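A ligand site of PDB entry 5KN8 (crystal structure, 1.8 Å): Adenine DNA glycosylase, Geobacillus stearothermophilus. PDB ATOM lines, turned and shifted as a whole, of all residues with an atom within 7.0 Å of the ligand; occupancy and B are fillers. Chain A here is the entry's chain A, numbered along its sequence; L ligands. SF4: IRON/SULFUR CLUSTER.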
ATOM      1  N   ARG A 152      -9.805 -22.508 -15.830  1.00  0.00           N
ATOM      2  CA  ARG A 152     -10.883 -22.669 -16.806  1.00  0.00           C
ATOM      3  C   ARG A 152     -11.219 -21.306 -17.436  1.00  0.00           C
ATOM      4  O   ARG A 152     -11.295 -21.188 -18.679  1.00  0.00           O
ATOM      5  CB  ARG A 152     -12.086 -23.324 -16.133  1.00  0.00           C
ATOM      6  CG  ARG A 152     -13.359 -23.358 -16.985  1.00  0.00           C
ATOM      7  CD  ARG A 152     -14.411 -24.256 -16.339  1.00  0.00           C
ATOM      8  NE  ARG A 152     -14.886 -23.693 -15.064  1.00  0.00           N
ATOM      9  CZ  ARG A 152     -14.474 -24.084 -13.856  1.00  0.00           C
ATOM     10  NH1 ARG A 152     -13.589 -25.066 -13.711  1.00  0.00           N
ATOM     11  NH2 ARG A 152     -14.966 -23.497 -12.780  1.00  0.00           N
ATOM     12  N   VAL A 153     -11.399 -20.274 -16.606  1.00  0.00           N
ATOM     13  CA  VAL A 153     -11.720 -18.923 -17.107  1.00  0.00           C
ATOM     14  C   VAL A 153     -10.627 -18.419 -18.042  1.00  0.00           C
ATOM     15  O   VAL A 153     -10.918 -17.951 -19.142  1.00  0.00           O
ATOM     16  CB  VAL A 153     -11.915 -17.875 -15.954  1.00  0.00           C
ATOM     17  CG1 VAL A 153     -12.101 -16.499 -16.530  1.00  0.00           C
ATOM     18  CG2 VAL A 153     -13.114 -18.240 -15.044  1.00  0.00           C
ATOM     19  N   LEU A 154      -9.364 -18.517 -17.614  1.00  0.00           N
ATOM     20  CA  LEU A 154      -8.286 -17.978 -18.440  1.00  0.00           C
ATOM     21  C   LEU A 154      -8.083 -18.787 -19.720  1.00  0.00           C
ATOM     22  O   LEU A 154      -7.747 -18.215 -20.756  1.00  0.00           O
ATOM     23  CB  LEU A 154      -6.957 -17.921 -17.668  1.00  0.00           C
ATOM     24  CG  LEU A 154      -6.959 -16.985 -16.443  1.00  0.00           C
ATOM     25  CD1 LEU A 154      -5.604 -17.022 -15.728  1.00  0.00           C
ATOM     26  CD2 LEU A 154      -7.360 -15.519 -16.823  1.00  0.00           C
ATOM     27  N   ARG A 156     -10.288 -20.174 -21.437  1.00  0.00           N
ATOM     28  CA  ARG A 156     -11.324 -19.771 -22.377  1.00  0.00           C
ATOM     29  C   ARG A 156     -11.072 -18.387 -22.925  1.00  0.00           C
ATOM     30  O   ARG A 156     -11.002 -18.208 -24.159  1.00  0.00           O
ATOM     31  CB  ARG A 156     -12.713 -19.868 -21.686  1.00  0.00           C
ATOM     32  CG  ARG A 156     -13.053 -21.324 -21.478  1.00  0.00           C
ATOM     33  CD  ARG A 156     -14.249 -21.538 -20.571  1.00  0.00           C
ATOM     34  NE  ARG A 156     -14.642 -22.943 -20.573  1.00  0.00           N
ATOM     35  CZ  ARG A 156     -15.634 -23.437 -19.830  1.00  0.00           C
ATOM     36  NH1 ARG A 156     -16.310 -22.616 -19.030  1.00  0.00           N
ATOM     37  NH2 ARG A 156     -15.945 -24.733 -19.897  1.00  0.00           N
ATOM     38  N   LEU A 157     -10.907 -17.408 -22.035  1.00  0.00           N
ATOM     39  CA  LEU A 157     -10.649 -16.031 -22.461  1.00  0.00           C
ATOM     40  C   LEU A 157      -9.510 -15.951 -23.475  1.00  0.00           C
ATOM     41  O   LEU A 157      -9.609 -15.261 -24.505  1.00  0.00           O
ATOM     42  CB  LEU A 157     -10.332 -15.146 -21.243  1.00  0.00           C
ATOM     43  CG  LEU A 157     -11.492 -14.784 -20.298  1.00  0.00           C
ATOM     44  CD1 LEU A 157     -10.949 -14.142 -19.029  1.00  0.00           C
ATOM     45  CD2 LEU A 157     -12.494 -13.855 -20.981  1.00  0.00           C
ATOM     46  N   LEU A 196     -16.375 -15.865 -10.946  1.00  0.00           N
ATOM     47  CA  LEU A 196     -16.855 -16.023 -12.326  1.00  0.00           C
ATOM     48  C   LEU A 196     -16.820 -17.508 -12.708  1.00  0.00           C
ATOM     49  O   LEU A 196     -17.768 -18.037 -13.280  1.00  0.00           O
ATOM     50  CB  LEU A 196     -16.011 -15.203 -13.300  1.00  0.00           C
ATOM     51  CG  LEU A 196     -16.542 -15.111 -14.744  1.00  0.00           C
ATOM     52  CD1 LEU A 196     -17.687 -14.116 -14.806  1.00  0.00           C
ATOM     53  CD2 LEU A 196     -15.431 -14.762 -15.762  1.00  0.00           C
ATOM     54  N   VAL A 200     -20.532 -18.592 -13.408  1.00  0.00           N
ATOM     55  CA  VAL A 200     -20.822 -18.253 -14.799  1.00  0.00           C
ATOM     56  C   VAL A 200     -20.038 -19.122 -15.759  1.00  0.00           C
ATOM     57  O   VAL A 200     -20.600 -19.827 -16.591  1.00  0.00           O
ATOM     58  CB  VAL A 200     -20.488 -16.772 -15.074  1.00  0.00           C
ATOM     59  CG1 VAL A 200     -20.754 -16.408 -16.539  1.00  0.00           C
ATOM     60  CG2 VAL A 200     -21.272 -15.849 -14.108  1.00  0.00           C
ATOM     61  N   CYS A 201     -18.722 -19.068 -15.631  1.00  0.00           N
ATOM     62  CA  CYS A 201     -17.855 -19.790 -16.529  1.00  0.00           C
ATOM     63  C   CYS A 201     -17.642 -21.186 -15.992  1.00  0.00           C
ATOM     64  O   CYS A 201     -16.549 -21.549 -15.570  1.00  0.00           O
ATOM     65  CB  CYS A 201     -16.533 -19.039 -16.681  1.00  0.00           C
ATOM     66  SG  CYS A 201     -15.527 -19.615 -18.061  1.00  0.00           S
ATOM     67  N   THR A 202     -18.718 -21.975 -15.994  1.00  0.00           N
ATOM     68  CA  THR A 202     -18.760 -23.274 -15.345  1.00  0.00           C
ATOM     69  C   THR A 202     -18.158 -24.386 -16.215  1.00  0.00           C
ATOM     70  O   THR A 202     -17.980 -24.197 -17.428  1.00  0.00           O
ATOM     71  CB  THR A 202     -20.211 -23.605 -14.945  1.00  0.00           C
ATOM     72  OG1 THR A 202     -21.055 -23.487 -16.089  1.00  0.00           O
ATOM     73  CG2 THR A 202     -20.701 -22.588 -13.872  1.00  0.00           C
ATOM     74  N   PRO A 206     -21.206 -23.258 -19.837  1.00  0.00           N
ATOM     75  CA  PRO A 206     -20.991 -21.921 -19.276  1.00  0.00           C
ATOM     76  C   PRO A 206     -22.070 -20.927 -19.700  1.00  0.00           C
ATOM     77  O   PRO A 206     -22.573 -21.020 -20.822  1.00  0.00           O
ATOM     78  CB  PRO A 206     -19.635 -21.512 -19.874  1.00  0.00           C
ATOM     79  CG  PRO A 206     -19.505 -22.337 -21.111  1.00  0.00           C
ATOM     80  CD  PRO A 206     -20.115 -23.659 -20.732  1.00  0.00           C
ATOM     81  N   SER A 207     -22.395 -19.991 -18.811  1.00  0.00           N
ATOM     82  CA  SER A 207     -23.445 -19.005 -19.057  1.00  0.00           C
ATOM     83  C   SER A 207     -22.939 -17.798 -19.869  1.00  0.00           C
ATOM     84  O   SER A 207     -23.085 -16.646 -19.453  1.00  0.00           O
ATOM     85  CB  SER A 207     -24.034 -18.572 -17.724  1.00  0.00           C
ATOM     86  OG  SER A 207     -24.646 -19.686 -17.096  1.00  0.00           O
ATOM     87  N   CYS A 208     -22.398 -18.077 -21.053  1.00  0.00           N
ATOM     88  CA  CYS A 208     -21.766 -17.050 -21.869  1.00  0.00           C
ATOM     89  C   CYS A 208     -22.667 -15.873 -22.174  1.00  0.00           C
ATOM     90  O   CYS A 208     -22.196 -14.722 -22.258  1.00  0.00           O
ATOM     91  CB  CYS A 208     -21.279 -17.648 -23.181  1.00  0.00           C
ATOM     92  SG  CYS A 208     -20.072 -18.987 -22.945  1.00  0.00           S
ATOM     93  N   LEU A 209     -23.963 -16.148 -22.362  1.00  0.00           N
ATOM     94  CA  LEU A 209     -24.895 -15.095 -22.777  1.00  0.00           C
ATOM     95  C   LEU A 209     -25.104 -14.027 -21.712  1.00  0.00           C
ATOM     96  O   LEU A 209     -25.517 -12.915 -22.027  1.00  0.00           O
ATOM     97  CB  LEU A 209     -26.241 -15.719 -23.159  1.00  0.00           C
ATOM     98  CG  LEU A 209     -26.159 -16.699 -24.343  1.00  0.00           C
ATOM     99  CD1 LEU A 209     -27.539 -17.315 -24.605  1.00  0.00           C
ATOM    100  CD2 LEU A 209     -25.621 -15.985 -25.597  1.00  0.00           C
ATOM    101  N   LEU A 210     -24.868 -14.393 -20.457  1.00  0.00           N
ATOM    102  CA  LEU A 210     -24.924 -13.431 -19.362  1.00  0.00           C
ATOM    103  C   LEU A 210     -23.554 -13.236 -18.685  1.00  0.00           C
ATOM    104  O   LEU A 210     -23.463 -12.917 -17.497  1.00  0.00           O
ATOM    105  CB  LEU A 210     -25.956 -13.866 -18.328  1.00  0.00           C
ATOM    106  CG  LEU A 210     -27.397 -13.846 -18.823  1.00  0.00           C
ATOM    107  CD1 LEU A 210     -28.365 -14.095 -17.688  1.00  0.00           C
ATOM    108  CD2 LEU A 210     -27.712 -12.542 -19.545  1.00  0.00           C
ATOM    109  N   CYS A 211     -22.489 -13.448 -19.450  1.00  0.00           N
ATOM    110  CA  CYS A 211     -21.147 -13.269 -18.913  1.00  0.00           C
ATOM    111  C   CYS A 211     -20.665 -11.819 -19.068  1.00  0.00           C
ATOM    112  O   CYS A 211     -20.718 -11.251 -20.161  1.00  0.00           O
ATOM    113  CB  CYS A 211     -20.160 -14.207 -19.603  1.00  0.00           C
ATOM    114  SG  CYS A 211     -18.473 -13.962 -19.013  1.00  0.00           S
ATOM    115  N   PRO A 212     -20.194 -11.227 -17.974  1.00  0.00           N
ATOM    116  CA  PRO A 212     -19.791  -9.824 -18.016  1.00  0.00           C
ATOM    117  C   PRO A 212     -18.553  -9.586 -18.877  1.00  0.00           C
ATOM    118  O   PRO A 212     -18.325  -8.445 -19.273  1.00  0.00           O
ATOM    119  CB  PRO A 212     -19.501  -9.498 -16.559  1.00  0.00           C
ATOM    120  CG  PRO A 212     -19.048 -10.786 -15.975  1.00  0.00           C
ATOM    121  CD  PRO A 212     -19.913 -11.828 -16.652  1.00  0.00           C
ATOM    122  N   VAL A 213     -17.785 -10.623 -19.176  1.00  0.00           N
ATOM    123  CA  VAL A 213     -16.553 -10.427 -19.949  1.00  0.00           C
ATOM    124  C   VAL A 213     -16.605 -11.176 -21.285  1.00  0.00           C
ATOM    125  O   VAL A 213     -15.591 -11.559 -21.845  1.00  0.00           O
ATOM    126  CB  VAL A 213     -15.328 -10.857 -19.140  1.00  0.00           C
ATOM    127  CG1 VAL A 213     -15.150  -9.917 -17.950  1.00  0.00           C
ATOM    128  CG2 VAL A 213     -15.465 -12.317 -18.675  1.00  0.00           C
ATOM    129  N   GLN A 214     -17.806 -11.348 -21.798  1.00  0.00           N
ATOM    130  CA  GLN A 214     -18.010 -12.061 -23.049  1.00  0.00           C
ATOM    131  C   GLN A 214     -17.296 -11.397 -24.221  1.00  0.00           C
ATOM    132  O   GLN A 214     -16.785 -12.086 -25.097  1.00  0.00           O
ATOM    133  CB  GLN A 214     -19.513 -12.164 -23.331  1.00  0.00           C
ATOM    134  CG  GLN A 214     -19.855 -12.896 -24.619  1.00  0.00           C
ATOM    135  CD  GLN A 214     -21.207 -12.468 -25.177  1.00  0.00           C
ATOM    136  OE1 GLN A 214     -21.266 -11.751 -26.171  1.00  0.00           O
ATOM    137  NE2 GLN A 214     -22.290 -12.900 -24.543  1.00  0.00           N
ATOM    138  N   ALA A 215     -17.255 -10.068 -24.231  1.00  0.00           N
ATOM    139  CA  ALA A 215     -16.666  -9.293 -25.324  1.00  0.00           C
ATOM    140  C   ALA A 215     -15.167  -9.518 -25.448  1.00  0.00           C
ATOM    141  O   ALA A 215     -14.574  -9.199 -26.471  1.00  0.00           O
ATOM    142  CB  ALA A 215     -16.964  -7.813 -25.158  1.00  0.00           C
ATOM    143  N   TYR A 216     -14.579 -10.049 -24.383  1.00  0.00           N
ATOM    144  CA  TYR A 216     -13.135 -10.260 -24.300  1.00  0.00           C
ATOM    145  C   TYR A 216     -12.732 -11.713 -24.575  1.00  0.00           C
ATOM    146  O   TYR A 216     -11.536 -12.047 -24.591  1.00  0.00           O
ATOM    147  CB  TYR A 216     -12.617  -9.838 -22.917  1.00  0.00           C
ATOM    148  CG  TYR A 216     -13.057  -8.450 -22.509  1.00  0.00           C
ATOM    149  CD1 TYR A 216     -12.350  -7.317 -22.907  1.00  0.00           C
ATOM    150  CD2 TYR A 216     -14.205  -8.259 -21.739  1.00  0.00           C
ATOM    151  CE1 TYR A 216     -12.760  -6.048 -22.549  1.00  0.00           C
ATOM    152  CE2 TYR A 216     -14.619  -6.998 -21.381  1.00  0.00           C
ATOM    153  CZ  TYR A 216     -13.904  -5.900 -21.785  1.00  0.00           C
ATOM    154  OH  TYR A 216     -14.342  -4.653 -21.414  1.00  0.00           O
ATOM    155  N   CYS A 217     -13.729 -12.580 -24.756  1.00  0.00           N
ATOM    156  CA  CYS A 217     -13.480 -14.017 -24.692  1.00  0.00           C
ATOM    157  C   CYS A 217     -13.245 -14.696 -26.046  1.00  0.00           C
ATOM    158  O   CYS A 217     -14.120 -14.715 -26.913  1.00  0.00           O
ATOM    159  CB  CYS A 217     -14.625 -14.707 -23.993  1.00  0.00           C
ATOM    160  SG  CYS A 217     -14.370 -16.482 -23.856  1.00  0.00           S
ATOM    161  N   GLN A 218     -12.044 -15.253 -26.232  1.00  0.00           N
ATOM    162  CA  GLN A 218     -11.723 -15.872 -27.514  1.00  0.00           C
ATOM    163  C   GLN A 218     -12.462 -17.208 -27.696  1.00  0.00           C
ATOM    164  O   GLN A 218     -12.882 -17.550 -28.801  1.00  0.00           O
ATOM    165  CB  GLN A 218     -10.204 -16.084 -27.620  1.00  0.00           C
ATOM    166  CG  GLN A 218      -9.422 -14.776 -27.716  1.00  0.00           C
ATOM    167  CD  GLN A 218      -7.940 -15.005 -27.857  1.00  0.00           C
ATOM    168  OE1 GLN A 218      -7.519 -15.899 -28.595  1.00  0.00           O
ATOM    169  NE2 GLN A 218      -7.136 -14.220 -27.156  1.00  0.00           N
ATOM    170  N   ALA A 219     -12.634 -17.954 -26.609  1.00  0.00           N
ATOM    171  CA  ALA A 219     -13.354 -19.237 -26.707  1.00  0.00           C
ATOM    172  C   ALA A 219     -14.803 -19.022 -27.138  1.00  0.00           C
ATOM    173  O   ALA A 219     -15.300 -19.730 -28.013  1.00  0.00           O
ATOM    174  CB  ALA A 219     -13.307 -19.982 -25.397  1.00  0.00           C
ATOM    175  N   PHE A 220     -15.466 -18.037 -26.547  1.00  0.00           N
ATOM    176  CA  PHE A 220     -16.842 -17.776 -26.976  1.00  0.00           C
ATOM    177  C   PHE A 220     -16.872 -17.399 -28.444  1.00  0.00           C
ATOM    178  O   PHE A 220     -17.688 -17.918 -29.216  1.00  0.00           O
ATOM    179  CB  PHE A 220     -17.493 -16.687 -26.140  1.00  0.00           C
ATOM    180  CG  PHE A 220     -18.891 -16.351 -26.597  1.00  0.00           C
ATOM    181  CD1 PHE A 220     -19.940 -17.234 -26.380  1.00  0.00           C
ATOM    182  CD2 PHE A 220     -19.162 -15.164 -27.269  1.00  0.00           C
ATOM    183  CE1 PHE A 220     -21.250 -16.934 -26.827  1.00  0.00           C
ATOM    184  CE2 PHE A 220     -20.456 -14.860 -27.700  1.00  0.00           C
ATOM    185  CZ  PHE A 220     -21.494 -15.748 -27.475  1.00  0.00           C
ATOM    186  N   ALA A 221     -15.959 -16.509 -28.829  1.00  0.00           N
ATOM    187  CA  ALA A 221     -15.881 -16.027 -30.204  1.00  0.00           C
ATOM    188  C   ALA A 221     -15.674 -17.172 -31.196  1.00  0.00           C
ATOM    189  O   ALA A 221     -16.155 -17.111 -32.335  1.00  0.00           O
ATOM    190  CB  ALA A 221     -14.763 -15.013 -30.348  1.00  0.00           C
ATOM    191  N   ALA A 225     -15.797 -22.940 -26.078  1.00  0.00           N
ATOM    192  CA  ALA A 225     -15.660 -22.832 -24.627  1.00  0.00           C
ATOM    193  C   ALA A 225     -15.805 -24.179 -23.921  1.00  0.00           C
ATOM    194  O   ALA A 225     -15.113 -24.447 -22.939  1.00  0.00           O
ATOM    195  CB  ALA A 225     -16.693 -21.829 -24.053  1.00  0.00           C
ATOM    196  N   GLU A 226     -16.685 -25.027 -24.430  1.00  0.00           N
ATOM    197  CA  GLU A 226     -16.960 -26.257 -23.718  1.00  0.00           C
ATOM    198  C   GLU A 226     -15.828 -27.271 -23.911  1.00  0.00           C
ATOM    199  O   GLU A 226     -15.751 -28.284 -23.232  1.00  0.00           O
ATOM    200  CB  GLU A 226     -18.290 -26.844 -24.140  1.00  0.00           C
ATOM    201  CG  GLU A 226     -19.463 -26.200 -23.385  1.00  0.00           C
ATOM    202  CD  GLU A 226     -20.650 -27.109 -23.329  1.00  0.00           C
ATOM    203  OE1 GLU A 226     -20.967 -27.615 -22.228  1.00  0.00           O
ATOM    204  OE2 GLU A 226     -21.239 -27.342 -24.399  1.00  0.00           O
HETATM  205 FE1  SF4 L   1     -18.348 -17.973 -21.710  1.00  0.00          FE
HETATM  206 FE2  SF4 L   1     -16.409 -18.242 -19.793  1.00  0.00          FE
HETATM  207 FE3  SF4 L   1     -17.592 -15.788 -20.173  1.00  0.00          FE
HETATM  208 FE4  SF4 L   1     -15.904 -16.799 -22.085  1.00  0.00          FE
HETATM  209  S1  SF4 L   1     -15.440 -16.283 -20.025  1.00  0.00           S
HETATM  210  S2  SF4 L   1     -17.894 -15.912 -22.333  1.00  0.00           S
HETATM  211  S3  SF4 L   1     -16.379 -18.922 -21.865  1.00  0.00           S
HETATM  212  S4  SF4 L   1     -18.541 -17.663 -19.535  1.00  0.00           S
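O of Leu 196 lies within hydrogen-bond range of N of Cys 201 (2.7 Å). The side-chain sulfur (SG) of Cys 217 lies close to the backbone NH (N) of Phe 220. The backbone carbonyl oxygen of Thr 202 lies within hydrogen-bond range of the guanidinium group of Arg 156, at 2.8 Å. O of Val 200 lies within hydrogen-bond range of N of Ser 207 (2.9 Å). The backbone carbonyl oxygen (O) of Cys 201 is in hydrogen-bond range of the guanidinium group (NE) of Arg 152, at 2.8 Å. The backbone NH (N) of Ala 219 sits close to the side-chain sulfur (SG) of Cys 217. O of Arg 156 lies close to SG of Cys 217, at 3.8 Å. The backbone NH (N) of Val 213 lies close to the side-chain sulfur (SG) of Cys 211 (3.4 Å).
Residues that only touch the ligand: Arg 156 (3.6 Å), Ala 225 (3.7 Å), Phe 220 (3.9 Å), Gln 214 (3.9 Å), Val 200 (3.9 Å) and Leu 157 (3.9 Å). Hydrophobic or aromatic side chains that line the ligand: Leu 157, Val 200, Phe 220 and Ala 225. Of the 27 residues printed, 10 come within 4 Å of the ligand. The nearest printed residue that does not touch the ligand is Pro 206 (4.02 Å).
SG of Cys 201 is bound to FE2 of the ligand. The side-chain sulfur of Cys 211 is bound to an iron atom (FE3) of the ligand (2.3 Å). The side-chain sulfur (SG) of Cys 217 is bound to an iron atom (FE4) of the ligand (2.4 Å). An iron atom (FE1) of the ligand is bound by the side-chain sulfur (SG) of Cys 208, 2.4 Å away.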
